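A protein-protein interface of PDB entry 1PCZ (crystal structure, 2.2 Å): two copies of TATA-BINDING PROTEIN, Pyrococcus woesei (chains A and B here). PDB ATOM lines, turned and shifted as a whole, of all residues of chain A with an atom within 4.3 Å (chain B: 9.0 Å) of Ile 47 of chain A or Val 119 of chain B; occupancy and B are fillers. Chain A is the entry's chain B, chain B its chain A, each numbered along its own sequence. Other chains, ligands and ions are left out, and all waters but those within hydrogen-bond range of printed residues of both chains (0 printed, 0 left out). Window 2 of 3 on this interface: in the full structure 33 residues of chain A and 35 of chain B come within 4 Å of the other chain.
Of the 21 printed residues of chain B, 7 touch a printed residue of chain A. Hydrophobic or aromatic side chains of chain B within 4 Å of the printed part of chain A: Val 119, Leu 122 and Leu 183.
No position is printed for both chains. Of the 12 pairs that touch across the chains among the printed residues, none has its exchanged pair printed and touching as well.
The side-chain amino group (NZ) of Lys 37 of chain A is in hydrogen-bond range of the side-chain hydroxyl (OG1) of Thr 123 of chain B (2.8 Å).
Of chain B, only Val 119 and Leu 122 come within 4 Å of Ile 47 of chain A. Of chain A, only Lys 37 (3.5 Å), Ile 47 (3.7 Å), His 49 (3.8 Å) and Ala 56 (3.7 Å) come within 4 Å of Val 119 of chain B. No residue of chain B comes within 4 Å of Ser 36 of chain A. Printed residues of chain B within 4 Å of Ala 56 of chain A: Asn 116 and Val 119. Of the printed residues of chain A, Asn 116 of chain B touches Ala 56. The nearest printed residue of chain A that does not touch Val 119 of chain B is Leu 58 of chain A (4.7 Å).
Among the printed residues, pairs that only touch across the chains: Lys 37 of chain A with Val 119 of chain B (3.5 Å), Lys 37 of chain A with Tyr 181 of chain B (3.9 Å), Lys 37 of chain A with Gly 182 of chain B (3.8 Å), Lys 37 of chain A with Leu 183 of chain B (3.0 Å), Phe 43 of chain A with Leu 122 of chain B (3.4 Å), Ile 47 of chain A with Val 119 of chain B (3.7 Å), Ile 47 of chain A with Leu 122 of chain B (3.8 Å), His 49 of chain A with Val 119 of chain B (3.8 Å), Ala 56 of chain A with Asn 116 of chain B (3.5 Å), Ala 56 of chain A with Val 119 of chain B (3.7 Å) and Leu 58 of chain A with Leu 122 of chain B (3.7 Å).
NH1 of Arg 113 of chain B lies within hydrogen-bond range of O of Leu 183 of chain B. OD1 of Asn 116 of chain B sits at hydrogen-bond distance from N of Val 119 of chain B (3.1 Å). The side-chain hydroxyl of Thr 123 of chain B lies within hydrogen-bond range of the backbone carbonyl oxygen of Val 119 of chain B, 2.8 Å away. N of Leu 183 of chain B is in hydrogen-bond range of O of Leu 178 of chain B (2.8 Å). N of His 49 of chain A lies within hydrogen-bond range of O of Asn 35 of chain A, at 2.7 Å. The backbone NH of Ile 47 of chain A sits at hydrogen-bond distance from the backbone carbonyl oxygen of Lys 37 of chain A, 2.9 Å away.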
ATOM      1  N   ASN A  35      -8.697 -11.489 -13.848  1.00  0.00           N
ATOM      2  CA  ASN A  35      -7.778 -12.276 -13.067  1.00  0.00           C
ATOM      3  C   ASN A  35      -7.500 -13.455 -13.960  1.00  0.00           C
ATOM      4  O   ASN A  35      -8.368 -13.871 -14.721  1.00  0.00           O
ATOM      5  CB  ASN A  35      -8.426 -12.743 -11.778  1.00  0.00           C
ATOM      6  CG  ASN A  35      -8.851 -11.600 -10.912  1.00  0.00           C
ATOM      7  OD1 ASN A  35     -10.009 -11.191 -10.938  1.00  0.00           O
ATOM      8  ND2 ASN A  35      -7.910 -11.054 -10.142  1.00  0.00           N
ATOM      9  N   SER A  36      -6.281 -13.961 -13.906  1.00  0.00           N
ATOM     10  CA  SER A  36      -5.897 -15.106 -14.699  1.00  0.00           C
ATOM     11  C   SER A  36      -4.855 -15.880 -13.939  1.00  0.00           C
ATOM     12  O   SER A  36      -4.269 -15.372 -12.999  1.00  0.00           O
ATOM     13  CB  SER A  36      -5.328 -14.664 -16.048  1.00  0.00           C
ATOM     14  OG  SER A  36      -4.526 -13.507 -15.894  1.00  0.00           O
ATOM     15  N   LYS A  37      -4.750 -17.157 -14.244  1.00  0.00           N
ATOM     16  CA  LYS A  37      -3.740 -17.997 -13.646  1.00  0.00           C
ATOM     17  C   LYS A  37      -3.066 -18.380 -14.928  1.00  0.00           C
ATOM     18  O   LYS A  37      -3.745 -18.773 -15.872  1.00  0.00           O
ATOM     19  CB  LYS A  37      -4.321 -19.271 -13.022  1.00  0.00           C
ATOM     20  CG  LYS A  37      -5.373 -19.050 -11.960  1.00  0.00           C
ATOM     21  CD  LYS A  37      -5.753 -20.378 -11.307  1.00  0.00           C
ATOM     22  CE  LYS A  37      -6.751 -20.185 -10.168  1.00  0.00           C
ATOM     23  NZ  LYS A  37      -6.721 -21.349  -9.242  1.00  0.00           N
ATOM     24  N   PHE A  43      -0.118 -25.810 -17.309  1.00  0.00           N
ATOM     25  CA  PHE A  43      -1.276 -25.727 -18.187  1.00  0.00           C
ATOM     26  C   PHE A  43      -0.999 -24.657 -19.213  1.00  0.00           C
ATOM     27  O   PHE A  43      -0.723 -23.509 -18.880  1.00  0.00           O
ATOM     28  CB  PHE A  43      -2.546 -25.390 -17.388  1.00  0.00           C
ATOM     29  CG  PHE A  43      -3.801 -25.411 -18.209  1.00  0.00           C
ATOM     30  CD1 PHE A  43      -4.195 -26.560 -18.861  1.00  0.00           C
ATOM     31  CD2 PHE A  43      -4.572 -24.262 -18.358  1.00  0.00           C
ATOM     32  CE1 PHE A  43      -5.336 -26.562 -19.653  1.00  0.00           C
ATOM     33  CE2 PHE A  43      -5.721 -24.259 -19.156  1.00  0.00           C
ATOM     34  CZ  PHE A  43      -6.098 -25.404 -19.798  1.00  0.00           C
ATOM     35  N   GLY A  45      -3.093 -23.147 -21.333  1.00  0.00           N
ATOM     36  CA  GLY A  45      -4.055 -22.091 -21.525  1.00  0.00           C
ATOM     37  C   GLY A  45      -4.016 -21.087 -20.415  1.00  0.00           C
ATOM     38  O   GLY A  45      -3.414 -21.340 -19.382  1.00  0.00           O
ATOM     39  N   ILE A  46      -4.582 -19.911 -20.649  1.00  0.00           N
ATOM     40  CA  ILE A  46      -4.661 -18.908 -19.599  1.00  0.00           C
ATOM     41  C   ILE A  46      -5.988 -19.224 -18.944  1.00  0.00           C
ATOM     42  O   ILE A  46      -6.972 -19.496 -19.635  1.00  0.00           O
ATOM     43  CB  ILE A  46      -4.815 -17.467 -20.126  1.00  0.00           C
ATOM     44  CG1 ILE A  46      -3.550 -17.009 -20.845  1.00  0.00           C
ATOM     45  CG2 ILE A  46      -5.161 -16.518 -18.984  1.00  0.00           C
ATOM     46  CD1 ILE A  46      -3.824 -15.812 -21.706  1.00  0.00           C
ATOM     47  N   ILE A  47      -5.994 -19.232 -17.619  1.00  0.00           N
ATOM     48  CA  ILE A  47      -7.204 -19.452 -16.867  1.00  0.00           C
ATOM     49  C   ILE A  47      -7.732 -18.046 -16.655  1.00  0.00           C
ATOM     50  O   ILE A  47      -7.350 -17.351 -15.718  1.00  0.00           O
ATOM     51  CB  ILE A  47      -6.903 -20.147 -15.544  1.00  0.00           C
ATOM     52  CG1 ILE A  47      -6.401 -21.553 -15.848  1.00  0.00           C
ATOM     53  CG2 ILE A  47      -8.124 -20.136 -14.648  1.00  0.00           C
ATOM     54  CD1 ILE A  47      -6.025 -22.326 -14.647  1.00  0.00           C
ATOM     55  N   CYS A  48      -8.552 -17.613 -17.598  1.00  0.00           N
ATOM     56  CA  CYS A  48      -9.146 -16.288 -17.582  1.00  0.00           C
ATOM     57  C   CYS A  48     -10.421 -16.135 -16.760  1.00  0.00           C
ATOM     58  O   CYS A  48     -11.514 -16.496 -17.199  1.00  0.00           O
ATOM     59  CB  CYS A  48      -9.436 -15.840 -19.003  1.00  0.00           C
ATOM     60  SG  CYS A  48      -9.666 -14.046 -19.127  1.00  0.00           S
ATOM     61  N   HIS A  49     -10.282 -15.519 -15.599  1.00  0.00           N
ATOM     62  CA  HIS A  49     -11.409 -15.282 -14.731  1.00  0.00           C
ATOM     63  C   HIS A  49     -12.115 -13.988 -15.028  1.00  0.00           C
ATOM     64  O   HIS A  49     -11.602 -12.904 -14.735  1.00  0.00           O
ATOM     65  CB  HIS A  49     -10.954 -15.269 -13.295  1.00  0.00           C
ATOM     66  CG  HIS A  49     -10.460 -16.591 -12.822  1.00  0.00           C
ATOM     67  ND1 HIS A  49      -9.126 -16.848 -12.598  1.00  0.00           N
ATOM     68  CD2 HIS A  49     -11.122 -17.735 -12.536  1.00  0.00           C
ATOM     69  CE1 HIS A  49      -8.985 -18.097 -12.188  1.00  0.00           C
ATOM     70  NE2 HIS A  49     -10.182 -18.654 -12.142  1.00  0.00           N
ATOM     71  N   ALA A  56     -14.738 -18.822 -16.046  1.00  0.00           N
ATOM     72  CA  ALA A  56     -13.302 -18.814 -16.312  1.00  0.00           C
ATOM     73  C   ALA A  56     -13.119 -19.410 -17.681  1.00  0.00           C
ATOM     74  O   ALA A  56     -13.681 -20.444 -17.996  1.00  0.00           O
ATOM     75  CB  ALA A  56     -12.512 -19.579 -15.279  1.00  0.00           C
ATOM     76  N   LEU A  57     -12.461 -18.662 -18.553  1.00  0.00           N
ATOM     77  CA  LEU A  57     -12.181 -19.127 -19.898  1.00  0.00           C
ATOM     78  C   LEU A  57     -10.786 -19.687 -19.853  1.00  0.00           C
ATOM     79  O   LEU A  57      -9.912 -19.144 -19.195  1.00  0.00           O
ATOM     80  CB  LEU A  57     -12.218 -17.955 -20.871  1.00  0.00           C
ATOM     81  CG  LEU A  57     -13.486 -17.095 -20.850  1.00  0.00           C
ATOM     82  CD1 LEU A  57     -13.328 -15.900 -21.782  1.00  0.00           C
ATOM     83  CD2 LEU A  57     -14.682 -17.932 -21.272  1.00  0.00           C
ATOM     84  N   LEU A  58     -10.602 -20.851 -20.434  1.00  0.00           N
ATOM     85  CA  LEU A  58      -9.271 -21.431 -20.491  1.00  0.00           C
ATOM     86  C   LEU A  58      -8.910 -21.026 -21.899  1.00  0.00           C
ATOM     87  O   LEU A  58      -9.487 -21.526 -22.868  1.00  0.00           O
ATOM     88  CB  LEU A  58      -9.314 -22.951 -20.355  1.00  0.00           C
ATOM     89  CG  LEU A  58     -10.139 -23.433 -19.153  1.00  0.00           C
ATOM     90  CD1 LEU A  58     -10.061 -24.954 -19.124  1.00  0.00           C
ATOM     91  CD2 LEU A  58      -9.675 -22.800 -17.818  1.00  0.00           C
ATOM     92  N   ARG B 113     -18.649 -22.840  -0.483  1.00  0.00           N
ATOM     93  CA  ARG B 113     -18.647 -21.982  -1.652  1.00  0.00           C
ATOM     94  C   ARG B 113     -18.619 -22.766  -2.925  1.00  0.00           C
ATOM     95  O   ARG B 113     -18.277 -23.944  -2.936  1.00  0.00           O
ATOM     96  CB  ARG B 113     -17.424 -21.073  -1.603  1.00  0.00           C
ATOM     97  CG  ARG B 113     -16.202 -21.794  -1.156  1.00  0.00           C
ATOM     98  CD  ARG B 113     -15.003 -21.144  -1.701  1.00  0.00           C
ATOM     99  NE  ARG B 113     -14.974 -21.268  -3.146  1.00  0.00           N
ATOM    100  CZ  ARG B 113     -13.990 -20.790  -3.891  1.00  0.00           C
ATOM    101  NH1 ARG B 113     -12.992 -20.155  -3.293  1.00  0.00           N
ATOM    102  NH2 ARG B 113     -13.965 -21.000  -5.209  1.00  0.00           N
ATOM    103  N   PHE B 115     -17.324 -23.660  -6.730  1.00  0.00           N
ATOM    104  CA  PHE B 115     -16.014 -23.814  -7.303  1.00  0.00           C
ATOM    105  C   PHE B 115     -16.132 -23.992  -8.784  1.00  0.00           C
ATOM    106  O   PHE B 115     -17.162 -24.419  -9.295  1.00  0.00           O
ATOM    107  CB  PHE B 115     -15.334 -25.061  -6.750  1.00  0.00           C
ATOM    108  CG  PHE B 115     -14.968 -24.952  -5.328  1.00  0.00           C
ATOM    109  CD1 PHE B 115     -15.901 -25.214  -4.347  1.00  0.00           C
ATOM    110  CD2 PHE B 115     -13.695 -24.546  -4.962  1.00  0.00           C
ATOM    111  CE1 PHE B 115     -15.562 -25.061  -3.036  1.00  0.00           C
ATOM    112  CE2 PHE B 115     -13.362 -24.395  -3.654  1.00  0.00           C
ATOM    113  CZ  PHE B 115     -14.291 -24.651  -2.691  1.00  0.00           C
ATOM    114  N   ASN B 116     -15.055 -23.667  -9.481  1.00  0.00           N
ATOM    115  CA  ASN B 116     -15.037 -23.865 -10.904  1.00  0.00           C
ATOM    116  C   ASN B 116     -14.175 -25.054 -10.883  1.00  0.00           C
ATOM    117  O   ASN B 116     -13.011 -24.959 -10.557  1.00  0.00           O
ATOM    118  CB  ASN B 116     -14.335 -22.754 -11.635  1.00  0.00           C
ATOM    119  CG  ASN B 116     -14.307 -22.988 -13.113  1.00  0.00           C
ATOM    120  OD1 ASN B 116     -13.984 -24.082 -13.569  1.00  0.00           O
ATOM    121  ND2 ASN B 116     -14.643 -21.963 -13.882  1.00  0.00           N
ATOM    122  N   LEU B 117     -14.804 -26.190 -11.106  1.00  0.00           N
ATOM    123  CA  LEU B 117     -14.154 -27.485 -11.094  1.00  0.00           C
ATOM    124  C   LEU B 117     -13.017 -27.604 -12.078  1.00  0.00           C
ATOM    125  O   LEU B 117     -12.024 -28.291 -11.822  1.00  0.00           O
ATOM    126  CB  LEU B 117     -15.213 -28.564 -11.318  1.00  0.00           C
ATOM    127  CG  LEU B 117     -15.789 -29.231 -10.059  1.00  0.00           C
ATOM    128  CD1 LEU B 117     -15.975 -28.285  -8.915  1.00  0.00           C
ATOM    129  CD2 LEU B 117     -17.033 -29.977 -10.408  1.00  0.00           C
ATOM    130  N   ASP B 118     -13.168 -26.972 -13.226  1.00  0.00           N
ATOM    131  CA  ASP B 118     -12.119 -27.019 -14.221  1.00  0.00           C
ATOM    132  C   ASP B 118     -10.889 -26.332 -13.679  1.00  0.00           C
ATOM    133  O   ASP B 118      -9.791 -26.855 -13.772  1.00  0.00           O
ATOM    134  CB  ASP B 118     -12.588 -26.357 -15.485  1.00  0.00           C
ATOM    135  CG  ASP B 118     -13.661 -27.147 -16.157  1.00  0.00           C
ATOM    136  OD1 ASP B 118     -14.816 -27.128 -15.678  1.00  0.00           O
ATOM    137  OD2 ASP B 118     -13.348 -27.803 -17.156  1.00  0.00           O
ATOM    138  N   VAL B 119     -11.090 -25.192 -13.035  1.00  0.00           N
ATOM    139  CA  VAL B 119      -9.988 -24.455 -12.449  1.00  0.00           C
ATOM    140  C   VAL B 119      -9.419 -25.255 -11.282  1.00  0.00           C
ATOM    141  O   VAL B 119      -8.216 -25.449 -11.185  1.00  0.00           O
ATOM    142  CB  VAL B 119     -10.430 -23.031 -12.035  1.00  0.00           C
ATOM    143  CG1 VAL B 119      -9.293 -22.288 -11.343  1.00  0.00           C
ATOM    144  CG2 VAL B 119     -10.875 -22.272 -13.284  1.00  0.00           C
ATOM    145  N   VAL B 120     -10.270 -25.766 -10.412  1.00  0.00           N
ATOM    146  CA  VAL B 120      -9.763 -26.570  -9.302  1.00  0.00           C
ATOM    147  C   VAL B 120      -8.966 -27.730  -9.873  1.00  0.00           C
ATOM    148  O   VAL B 120      -7.849 -27.976  -9.459  1.00  0.00           O
ATOM    149  CB  VAL B 120     -10.909 -27.158  -8.414  1.00  0.00           C
ATOM    150  CG1 VAL B 120     -10.317 -28.065  -7.343  1.00  0.00           C
ATOM    151  CG2 VAL B 120     -11.703 -26.024  -7.763  1.00  0.00           C
ATOM    152  N   ALA B 121      -9.519 -28.399 -10.873  1.00  0.00           N
ATOM    153  CA  ALA B 121      -8.850 -29.532 -11.475  1.00  0.00           C
ATOM    154  C   ALA B 121      -7.538 -29.128 -12.124  1.00  0.00           C
ATOM    155  O   ALA B 121      -6.616 -29.917 -12.218  1.00  0.00           O
ATOM    156  CB  ALA B 121      -9.736 -30.158 -12.476  1.00  0.00           C
ATOM    157  N   LEU B 122      -7.479 -27.907 -12.635  1.00  0.00           N
ATOM    158  CA  LEU B 122      -6.270 -27.428 -13.273  1.00  0.00           C
ATOM    159  C   LEU B 122      -5.287 -26.996 -12.214  1.00  0.00           C
ATOM    160  O   LEU B 122      -4.092 -27.164 -12.359  1.00  0.00           O
ATOM    161  CB  LEU B 122      -6.576 -26.239 -14.196  1.00  0.00           C
ATOM    162  CG  LEU B 122      -7.194 -26.601 -15.524  1.00  0.00           C
ATOM    163  CD1 LEU B 122      -7.554 -25.371 -16.257  1.00  0.00           C
ATOM    164  CD2 LEU B 122      -6.244 -27.420 -16.311  1.00  0.00           C
ATOM    165  N   THR B 123      -5.804 -26.472 -11.125  1.00  0.00           N
ATOM    166  CA  THR B 123      -4.963 -25.960 -10.068  1.00  0.00           C
ATOM    167  C   THR B 123      -4.484 -26.993  -9.057  1.00  0.00           C
ATOM    168  O   THR B 123      -3.289 -27.076  -8.749  1.00  0.00           O
ATOM    169  CB  THR B 123      -5.707 -24.835  -9.358  1.00  0.00           C
ATOM    170  OG1 THR B 123      -6.117 -23.872 -10.332  1.00  0.00           O
ATOM    171  CG2 THR B 123      -4.838 -24.176  -8.325  1.00  0.00           C
ATOM    172  N   LEU B 124      -5.445 -27.749  -8.532  1.00  0.00           N
ATOM    173  CA  LEU B 124      -5.238 -28.772  -7.524  1.00  0.00           C
ATOM    174  C   LEU B 124      -4.444 -29.931  -8.023  1.00  0.00           C
ATOM    175  O   LEU B 124      -4.880 -30.659  -8.913  1.00  0.00           O
ATOM    176  CB  LEU B 124      -6.571 -29.285  -7.014  1.00  0.00           C
ATOM    177  CG  LEU B 124      -6.693 -29.308  -5.501  1.00  0.00           C
ATOM    178  CD1 LEU B 124      -6.392 -27.908  -4.970  1.00  0.00           C
ATOM    179  CD2 LEU B 124      -8.106 -29.752  -5.122  1.00  0.00           C
ATOM    180  N   PRO B 125      -3.304 -30.185  -7.369  1.00  0.00           N
ATOM    181  CA  PRO B 125      -2.409 -31.273  -7.731  1.00  0.00           C
ATOM    182  C   PRO B 125      -3.004 -32.687  -7.689  1.00  0.00           C
ATOM    183  O   PRO B 125      -3.097 -33.337  -8.745  1.00  0.00           O
ATOM    184  CB  PRO B 125      -1.234 -31.076  -6.767  1.00  0.00           C
ATOM    185  CG  PRO B 125      -1.856 -30.488  -5.589  1.00  0.00           C
ATOM    186  CD  PRO B 125      -2.768 -29.459  -6.207  1.00  0.00           C
ATOM    187  N   CYS B 127      -6.022 -34.405  -7.727  1.00  0.00           N
ATOM    188  CA  CYS B 127      -7.460 -34.517  -7.943  1.00  0.00           C
ATOM    189  C   CYS B 127      -7.761 -35.041  -9.349  1.00  0.00           C
ATOM    190  O   CYS B 127      -6.907 -35.037 -10.224  1.00  0.00           O
ATOM    191  CB  CYS B 127      -8.163 -33.183  -7.668  1.00  0.00           C
ATOM    192  SG  CYS B 127      -8.018 -31.973  -8.959  1.00  0.00           S
ATOM    193  N   TYR B 129     -10.631 -35.225 -12.548  1.00  0.00           N
ATOM    194  CA  TYR B 129     -11.734 -34.485 -13.057  1.00  0.00           C
ATOM    195  C   TYR B 129     -11.949 -34.769 -14.509  1.00  0.00           C
ATOM    196  O   TYR B 129     -11.113 -34.432 -15.328  1.00  0.00           O
ATOM    197  CB  TYR B 129     -11.456 -32.999 -12.873  1.00  0.00           C
ATOM    198  CG  TYR B 129     -12.540 -32.121 -13.414  1.00  0.00           C
ATOM    199  CD1 TYR B 129     -13.818 -32.126 -12.839  1.00  0.00           C
ATOM    200  CD2 TYR B 129     -12.295 -31.250 -14.481  1.00  0.00           C
ATOM    201  CE1 TYR B 129     -14.824 -31.271 -13.311  1.00  0.00           C
ATOM    202  CE2 TYR B 129     -13.292 -30.397 -14.961  1.00  0.00           C
ATOM    203  CZ  TYR B 129     -14.546 -30.408 -14.366  1.00  0.00           C
ATOM    204  OH  TYR B 129     -15.511 -29.534 -14.788  1.00  0.00           O
ATOM    205  N   VAL B 137     -15.093 -33.154  -8.993  1.00  0.00           N
ATOM    206  CA  VAL B 137     -13.654 -33.302  -8.910  1.00  0.00           C
ATOM    207  C   VAL B 137     -13.477 -34.316  -7.791  1.00  0.00           C
ATOM    208  O   VAL B 137     -14.053 -34.178  -6.707  1.00  0.00           O
ATOM    209  CB  VAL B 137     -12.948 -31.957  -8.476  1.00  0.00           C
ATOM    210  CG1 VAL B 137     -11.516 -32.226  -8.060  1.00  0.00           C
ATOM    211  CG2 VAL B 137     -12.987 -30.928  -9.595  1.00  0.00           C
ATOM    212  N   LEU B 150     -16.023 -33.264  -5.081  1.00  0.00           N
ATOM    213  CA  LEU B 150     -16.326 -31.844  -4.964  1.00  0.00           C
ATOM    214  C   LEU B 150     -17.135 -31.431  -6.161  1.00  0.00           C
ATOM    215  O   LEU B 150     -16.776 -31.718  -7.307  1.00  0.00           O
ATOM    216  CB  LEU B 150     -15.030 -31.033  -4.979  1.00  0.00           C
ATOM    217  CG  LEU B 150     -14.832 -29.668  -4.318  1.00  0.00           C
ATOM    218  CD1 LEU B 150     -13.780 -28.882  -5.098  1.00  0.00           C
ATOM    219  CD2 LEU B 150     -16.095 -28.903  -4.200  1.00  0.00           C
ATOM    220  N   LEU B 178      -6.975 -26.608  -1.390  1.00  0.00           N
ATOM    221  CA  LEU B 178      -7.614 -25.623  -2.256  1.00  0.00           C
ATOM    222  C   LEU B 178      -7.050 -24.286  -1.849  1.00  0.00           C
ATOM    223  O   LEU B 178      -6.640 -23.493  -2.681  1.00  0.00           O
ATOM    224  CB  LEU B 178      -9.141 -25.621  -2.078  1.00  0.00           C
ATOM    225  CG  LEU B 178      -9.897 -26.819  -2.661  1.00  0.00           C
ATOM    226  CD1 LEU B 178     -11.309 -26.825  -2.159  1.00  0.00           C
ATOM    227  CD2 LEU B 178      -9.880 -26.773  -4.166  1.00  0.00           C
ATOM    228  N   TYR B 181      -3.638 -23.542  -2.932  1.00  0.00           N
ATOM    229  CA  TYR B 181      -3.577 -23.225  -4.345  1.00  0.00           C
ATOM    230  C   TYR B 181      -4.458 -22.061  -4.713  1.00  0.00           C
ATOM    231  O   TYR B 181      -4.838 -21.903  -5.866  1.00  0.00           O
ATOM    232  CB  TYR B 181      -3.900 -24.451  -5.165  1.00  0.00           C
ATOM    233  CG  TYR B 181      -2.835 -25.491  -5.018  1.00  0.00           C
ATOM    234  CD1 TYR B 181      -2.880 -26.414  -3.982  1.00  0.00           C
ATOM    235  CD2 TYR B 181      -1.757 -25.532  -5.887  1.00  0.00           C
ATOM    236  CE1 TYR B 181      -1.876 -27.351  -3.811  1.00  0.00           C
ATOM    237  CE2 TYR B 181      -0.736 -26.468  -5.734  1.00  0.00           C
ATOM    238  CZ  TYR B 181      -0.800 -27.376  -4.694  1.00  0.00           C
ATOM    239  OH  TYR B 181       0.202 -28.318  -4.539  1.00  0.00           O
ATOM    240  N   GLY B 182      -4.747 -21.224  -3.727  1.00  0.00           N
ATOM    241  CA  GLY B 182      -5.568 -20.057  -3.963  1.00  0.00           C
ATOM    242  C   GLY B 182      -6.846 -20.374  -4.687  1.00  0.00           C
ATOM    243  O   GLY B 182      -7.128 -19.823  -5.752  1.00  0.00           O
ATOM    244  N   LEU B 183      -7.602 -21.309  -4.129  1.00  0.00           N
ATOM    245  CA  LEU B 183      -8.864 -21.708  -4.713  1.00  0.00           C
ATOM    246  C   LEU B 183     -10.002 -21.442  -3.748  1.00  0.00           C
ATOM    247  O   LEU B 183     -11.145 -21.811  -4.008  1.00  0.00           O
ATOM    248  CB  LEU B 183      -8.814 -23.167  -5.136  1.00  0.00           C
ATOM    249  CG  LEU B 183      -7.936 -23.429  -6.355  1.00  0.00           C
ATOM    250  CD1 LEU B 183      -7.564 -24.900  -6.394  1.00  0.00           C
ATOM    251  CD2 LEU B 183      -8.651 -23.017  -7.637  1.00  0.00           C
ATOM    252  N   LEU B 184      -9.682 -20.775  -2.647  1.00  0.00           N
ATOM    253  CA  LEU B 184     -10.679 -20.417  -1.654  1.00  0.00           C
ATOM    254  C   LEU B 184     -10.604 -18.904  -1.464  1.00  0.00           C
ATOM    255  O   LEU B 184      -9.741 -18.467  -0.676  1.00  0.00           O
ATOM    256  CB  LEU B 184     -10.415 -21.117  -0.320  1.00  0.00           C
ATOM    257  CG  LEU B 184     -10.488 -22.636  -0.206  1.00  0.00           C
ATOM    258  CD1 LEU B 184     -10.223 -22.991   1.256  1.00  0.00           C
ATOM    259  CD2 LEU B 184     -11.843 -23.162  -0.678  1.00  0.00           C
